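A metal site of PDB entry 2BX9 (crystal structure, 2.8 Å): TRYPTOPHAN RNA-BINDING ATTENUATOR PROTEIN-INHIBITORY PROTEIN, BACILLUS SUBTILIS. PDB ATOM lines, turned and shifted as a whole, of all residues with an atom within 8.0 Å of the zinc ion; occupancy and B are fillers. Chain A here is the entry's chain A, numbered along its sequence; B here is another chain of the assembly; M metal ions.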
ATOM      1  N   VAL A  10      10.177 -27.349  10.494  1.00  0.00           N
ATOM      2  CA  VAL A  10       9.829 -27.174  11.899  1.00  0.00           C
ATOM      3  C   VAL A  10       8.447 -27.807  12.144  1.00  0.00           C
ATOM      4  O   VAL A  10       7.565 -27.710  11.302  1.00  0.00           O
ATOM      5  CB  VAL A  10       9.849 -25.664  12.250  1.00  0.00           C
ATOM      6  CG1 VAL A  10       9.072 -25.368  13.497  1.00  0.00           C
ATOM      7  CG2 VAL A  10      11.279 -25.212  12.397  1.00  0.00           C
ATOM      8  N   ALA A  11       8.283 -28.486  13.283  1.00  0.00           N
ATOM      9  CA  ALA A  11       6.990 -29.042  13.687  1.00  0.00           C
ATOM     10  C   ALA A  11       5.983 -27.917  13.752  1.00  0.00           C
ATOM     11  O   ALA A  11       6.268 -26.852  14.303  1.00  0.00           O
ATOM     12  CB  ALA A  11       7.103 -29.718  15.031  1.00  0.00           C
ATOM     13  N   CYS A  12       4.800 -28.140  13.178  1.00  0.00           N
ATOM     14  CA  CYS A  12       3.764 -27.117  13.194  1.00  0.00           C
ATOM     15  C   CYS A  12       3.183 -26.955  14.605  1.00  0.00           C
ATOM     16  O   CYS A  12       2.816 -27.932  15.253  1.00  0.00           O
ATOM     17  CB  CYS A  12       2.656 -27.478  12.229  1.00  0.00           C
ATOM     18  SG  CYS A  12       1.270 -26.325  12.150  1.00  0.00           S
ATOM     19  N   PRO A  13       3.129 -25.696  15.070  1.00  0.00           N
ATOM     20  CA  PRO A  13       2.599 -25.392  16.417  1.00  0.00           C
ATOM     21  C   PRO A  13       1.124 -25.760  16.563  1.00  0.00           C
ATOM     22  O   PRO A  13       0.741 -26.332  17.588  1.00  0.00           O
ATOM     23  CB  PRO A  13       2.800 -23.875  16.552  1.00  0.00           C
ATOM     24  CG  PRO A  13       2.949 -23.369  15.142  1.00  0.00           C
ATOM     25  CD  PRO A  13       3.586 -24.493  14.359  1.00  0.00           C
ATOM     26  N   LYS A  14       0.323 -25.451  15.543  1.00  0.00           N
ATOM     27  CA  LYS A  14      -1.124 -25.667  15.573  1.00  0.00           C
ATOM     28  C   LYS A  14      -1.519 -27.144  15.678  1.00  0.00           C
ATOM     29  O   LYS A  14      -2.232 -27.513  16.602  1.00  0.00           O
ATOM     30  CB  LYS A  14      -1.800 -25.006  14.348  1.00  0.00           C
ATOM     31  CG  LYS A  14      -3.327 -25.235  14.227  1.00  0.00           C
ATOM     32  CD  LYS A  14      -4.160 -24.379  15.180  1.00  0.00           C
ATOM     33  CE  LYS A  14      -5.642 -24.564  14.938  1.00  0.00           C
ATOM     34  NZ  LYS A  14      -6.469 -23.718  15.845  1.00  0.00           N
ATOM     35  N   CYS A  15      -1.048 -27.967  14.754  1.00  0.00           N
ATOM     36  CA  CYS A  15      -1.430 -29.376  14.701  1.00  0.00           C
ATOM     37  C   CYS A  15      -0.431 -30.327  15.357  1.00  0.00           C
ATOM     38  O   CYS A  15      -0.643 -31.551  15.371  1.00  0.00           O
ATOM     39  CB  CYS A  15      -1.702 -29.803  13.254  1.00  0.00           C
ATOM     40  SG  CYS A  15      -0.271 -29.686  12.172  1.00  0.00           S
ATOM     41  N   GLU A  16       0.647 -29.759  15.919  1.00  0.00           N
ATOM     42  CA  GLU A  16       1.721 -30.508  16.569  1.00  0.00           C
ATOM     43  C   GLU A  16       2.138 -31.749  15.759  1.00  0.00           C
ATOM     44  O   GLU A  16       2.111 -32.876  16.255  1.00  0.00           O
ATOM     45  CB  GLU A  16       1.340 -30.854  18.019  1.00  0.00           C
ATOM     46  CG  GLU A  16       1.360 -29.666  18.983  1.00  0.00           C
ATOM     47  CD  GLU A  16       1.158 -30.071  20.437  1.00  0.00           C
ATOM     48  OE1 GLU A  16       0.650 -31.199  20.697  1.00  0.00           O
ATOM     49  OE2 GLU A  16       1.510 -29.274  21.334  1.00  0.00           O
ATOM     50  N   ARG A  17       2.491 -31.512  14.498  1.00  0.00           N
ATOM     51  CA  ARG A  17       3.096 -32.520  13.643  1.00  0.00           C
ATOM     52  C   ARG A  17       2.044 -33.415  12.962  1.00  0.00           C
ATOM     53  O   ARG A  17       2.329 -34.074  11.972  1.00  0.00           O
ATOM     54  CB  ARG A  17       4.117 -33.350  14.453  1.00  0.00           C
ATOM     55  CG  ARG A  17       5.077 -34.243  13.681  1.00  0.00           C
ATOM     56  CD  ARG A  17       6.274 -33.528  13.061  1.00  0.00           C
ATOM     57  NE  ARG A  17       7.272 -33.084  14.046  1.00  0.00           N
ATOM     58  CZ  ARG A  17       8.515 -32.725  13.739  1.00  0.00           C
ATOM     59  NH1 ARG A  17       8.923 -32.764  12.471  1.00  0.00           N
ATOM     60  NH2 ARG A  17       9.349 -32.326  14.687  1.00  0.00           N
ATOM     61  N   ALA A  18       0.815 -33.411  13.497  1.00  0.00           N
ATOM     62  CA  ALA A  18      -0.238 -34.322  13.030  1.00  0.00           C
ATOM     63  C   ALA A  18      -0.904 -33.909  11.714  1.00  0.00           C
ATOM     64  O   ALA A  18      -1.574 -34.734  11.075  1.00  0.00           O
ATOM     65  CB  ALA A  18      -1.272 -34.556  14.124  1.00  0.00           C
ATOM     66  N   GLY A  19      -0.731 -32.651  11.299  1.00  0.00           N
ATOM     67  CA  GLY A  19      -1.292 -32.150  10.034  1.00  0.00           C
ATOM     68  C   GLY A  19      -2.796 -31.954  10.050  1.00  0.00           C
ATOM     69  O   GLY A  19      -3.369 -31.447   9.090  1.00  0.00           O
ATOM     70  N   GLU A  20      -3.410 -32.341  11.161  1.00  0.00           N
ATOM     71  CA  GLU A  20      -4.862 -32.409  11.316  1.00  0.00           C
ATOM     72  C   GLU A  20      -5.272 -31.868  12.686  1.00  0.00           C
ATOM     73  O   GLU A  20      -4.585 -32.113  13.694  1.00  0.00           O
ATOM     74  CB  GLU A  20      -5.326 -33.869  11.115  1.00  0.00           C
ATOM     75  CG  GLU A  20      -6.354 -34.423  12.107  1.00  0.00           C
ATOM     76  CD  GLU A  20      -5.718 -35.157  13.282  1.00  0.00           C
ATOM     77  OE1 GLU A  20      -5.147 -36.257  13.088  1.00  0.00           O
ATOM     78  OE2 GLU A  20      -5.798 -34.646  14.419  1.00  0.00           O
ATOM     79  N   ILE A  21      -6.371 -31.130  12.729  1.00  0.00           N
ATOM     80  CA  ILE A  21      -6.984 -30.722  13.974  1.00  0.00           C
ATOM     81  C   ILE A  21      -8.382 -31.326  14.001  1.00  0.00           C
ATOM     82  O   ILE A  21      -9.209 -31.023  13.142  1.00  0.00           O
ATOM     83  CB  ILE A  21      -7.071 -29.171  14.078  1.00  0.00           C
ATOM     84  CG1 ILE A  21      -5.668 -28.546  14.125  1.00  0.00           C
ATOM     85  CG2 ILE A  21      -7.902 -28.748  15.301  1.00  0.00           C
ATOM     86  CD1 ILE A  21      -4.908 -28.777  15.422  1.00  0.00           C
ATOM     87  N   PRO A  25      -8.621 -30.250   8.424  1.00  0.00           N
ATOM     88  CA  PRO A  25      -7.259 -30.091   7.898  1.00  0.00           C
ATOM     89  C   PRO A  25      -6.626 -28.798   8.391  1.00  0.00           C
ATOM     90  O   PRO A  25      -7.290 -27.745   8.387  1.00  0.00           O
ATOM     91  CB  PRO A  25      -7.476 -30.047   6.374  1.00  0.00           C
ATOM     92  CG  PRO A  25      -8.941 -29.735   6.201  1.00  0.00           C
ATOM     93  CD  PRO A  25      -9.626 -30.392   7.358  1.00  0.00           C
ATOM     94  N   CYS A  26      -5.374 -28.879   8.807  1.00  0.00           N
ATOM     95  CA  CYS A  26      -4.712 -27.748   9.451  1.00  0.00           C
ATOM     96  C   CYS A  26      -4.401 -26.628   8.450  1.00  0.00           C
ATOM     97  O   CYS A  26      -3.736 -26.881   7.448  1.00  0.00           O
ATOM     98  CB  CYS A  26      -3.447 -28.224  10.157  1.00  0.00           C
ATOM     99  SG  CYS A  26      -2.529 -26.907  10.987  1.00  0.00           S
ATOM    100  N   PRO A  27      -4.888 -25.406   8.703  1.00  0.00           N
ATOM    101  CA  PRO A  27      -4.600 -24.271   7.837  1.00  0.00           C
ATOM    102  C   PRO A  27      -3.216 -23.635   8.047  1.00  0.00           C
ATOM    103  O   PRO A  27      -2.704 -22.998   7.132  1.00  0.00           O
ATOM    104  CB  PRO A  27      -5.704 -23.285   8.188  1.00  0.00           C
ATOM    105  CG  PRO A  27      -6.637 -24.052   9.062  1.00  0.00           C
ATOM    106  CD  PRO A  27      -5.785 -25.017   9.799  1.00  0.00           C
ATOM    107  N   ALA A  28      -2.626 -23.799   9.224  1.00  0.00           N
ATOM    108  CA  ALA A  28      -1.286 -23.250   9.484  1.00  0.00           C
ATOM    109  C   ALA A  28      -0.249 -23.833   8.513  1.00  0.00           C
ATOM    110  O   ALA A  28       0.447 -23.094   7.800  1.00  0.00           O
ATOM    111  CB  ALA A  28      -0.879 -23.509  10.943  1.00  0.00           C
ATOM    112  N   CYS A  29      -0.160 -25.157   8.466  1.00  0.00           N
ATOM    113  CA  CYS A  29       0.834 -25.852   7.656  1.00  0.00           C
ATOM    114  C   CYS A  29       0.191 -26.528   6.447  1.00  0.00           C
ATOM    115  O   CYS A  29       0.809 -27.401   5.821  1.00  0.00           O
ATOM    116  CB  CYS A  29       1.503 -26.919   8.501  1.00  0.00           C
ATOM    117  SG  CYS A  29       0.327 -28.195   8.965  1.00  0.00           S
ATOM    118  N   SER A  30      -1.046 -26.132   6.158  1.00  0.00           N
ATOM    119  CA  SER A  30      -1.812 -26.689   5.040  1.00  0.00           C
ATOM    120  C   SER A  30      -1.603 -28.198   4.826  1.00  0.00           C
ATOM    121  O   SER A  30      -1.095 -28.615   3.796  1.00  0.00           O
ATOM    122  CB  SER A  30      -1.502 -25.929   3.736  1.00  0.00           C
ATOM    123  OG  SER A  30      -0.126 -26.024   3.414  1.00  0.00           O
ATOM    124  N   GLY A  31      -1.980 -28.997   5.814  1.00  0.00           N
ATOM    125  CA  GLY A  31      -1.937 -30.451   5.687  1.00  0.00           C
ATOM    126  C   GLY A  31      -0.622 -31.132   6.022  1.00  0.00           C
ATOM    127  O   GLY A  31      -0.615 -32.261   6.514  1.00  0.00           O
ATOM    128  N   LYS A  32       0.491 -30.455   5.753  1.00  0.00           N
ATOM    129  CA  LYS A  32       1.805 -31.091   5.836  1.00  0.00           C
ATOM    130  C   LYS A  32       2.324 -31.369   7.264  1.00  0.00           C
ATOM    131  O   LYS A  32       3.142 -32.262   7.447  1.00  0.00           O
ATOM    132  CB  LYS A  32       2.841 -30.299   5.025  1.00  0.00           C
ATOM    133  CG  LYS A  32       2.663 -30.399   3.502  1.00  0.00           C
ATOM    134  CD  LYS A  32       3.723 -29.575   2.772  1.00  0.00           C
ATOM    135  CE  LYS A  32       3.686 -29.820   1.267  1.00  0.00           C
ATOM    136  NZ  LYS A  32       4.720 -29.022   0.529  1.00  0.00           N
ATOM    137  N   GLY A  33       1.858 -30.619   8.255  1.00  0.00           N
ATOM    138  CA  GLY A  33       2.229 -30.876   9.662  1.00  0.00           C
ATOM    139  C   GLY A  33       3.555 -30.246  10.051  1.00  0.00           C
ATOM    140  O   GLY A  33       4.030 -30.387  11.188  1.00  0.00           O
ATOM    141  N   VAL A  34       4.137 -29.522   9.105  1.00  0.00           N
ATOM    142  CA  VAL A  34       5.496 -29.010   9.212  1.00  0.00           C
ATOM    143  C   VAL A  34       5.552 -27.657   8.495  1.00  0.00           C
ATOM    144  O   VAL A  34       4.859 -27.455   7.495  1.00  0.00           O
ATOM    145  CB  VAL A  34       6.497 -30.003   8.570  1.00  0.00           C
ATOM    146  CG1 VAL A  34       7.836 -29.352   8.391  1.00  0.00           C
ATOM    147  CG2 VAL A  34       6.665 -31.283   9.415  1.00  0.00           C
ATOM    148  N   ILE A  35       6.379 -26.742   9.013  1.00  0.00           N
ATOM    149  CA  ILE A  35       6.618 -25.451   8.372  1.00  0.00           C
ATOM    150  C   ILE A  35       8.073 -25.387   7.935  1.00  0.00           C
ATOM    151  O   ILE A  35       8.955 -25.809   8.682  1.00  0.00           O
ATOM    152  CB  ILE A  35       6.268 -24.301   9.340  1.00  0.00           C
ATOM    153  CG1 ILE A  35       4.771 -24.293   9.613  1.00  0.00           C
ATOM    154  CG2 ILE A  35       6.694 -22.946   8.765  1.00  0.00           C
ATOM    155  CD1 ILE A  35       4.407 -23.548  10.844  1.00  0.00           C
ATOM    156  N   ALA B  28      -2.198 -19.188  13.621  1.00  0.00           N
ATOM    157  CA  ALA B  28      -1.143 -20.146  13.324  1.00  0.00           C
ATOM    158  C   ALA B  28      -0.050 -20.225  14.388  1.00  0.00           C
ATOM    159  O   ALA B  28       0.207 -21.314  14.905  1.00  0.00           O
ATOM    160  CB  ALA B  28      -0.569 -19.882  11.917  1.00  0.00           C
HETATM  161 ZN    ZN M   1      -0.331 -27.638  11.096  1.00  0.00          ZN
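SG of Cys 29 lies close to N of Gly 33, 3.0 Å away.
SG of Cys 15 lies close to N of Gly 19 (3.1 Å).
SG of Cys 26 lies close to N of Ala 28 of chain A (3.6 Å).
The backbone carbonyl oxygen (O) of Gly 19 sits at hydrogen-bond distance from the backbone NH (N) of Cys 26 (3.3 Å).
The backbone NH (N) of Gly 31 sits at hydrogen-bond distance from the backbone carbonyl oxygen (O) of Cys 26 (3.2 Å).
The backbone NH (N) of Cys 12 is in hydrogen-bond range of the backbone carbonyl oxygen (O) of Gly 33, 3.1 Å away.
The side-chain sulfur (SG) of Cys 12 lies close to the backbone NH (N) of Lys 14, 3.6 Å away.
The zinc ion is bound by SG of Cys 29 (2.3 Å).
The side-chain sulfur (SG) of Cys 15 binds the zinc ion.
The zinc ion is bound by SG of Cys 26, 2.3 Å away.
SG of Cys 12 is bound to the zinc ion, at 2.3 Å.
The zinc ion has four donor atoms within binding distance.
Within 4 Å of the zinc ion: Cys 12, Cys 15, Cys 26 and Cys 29.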
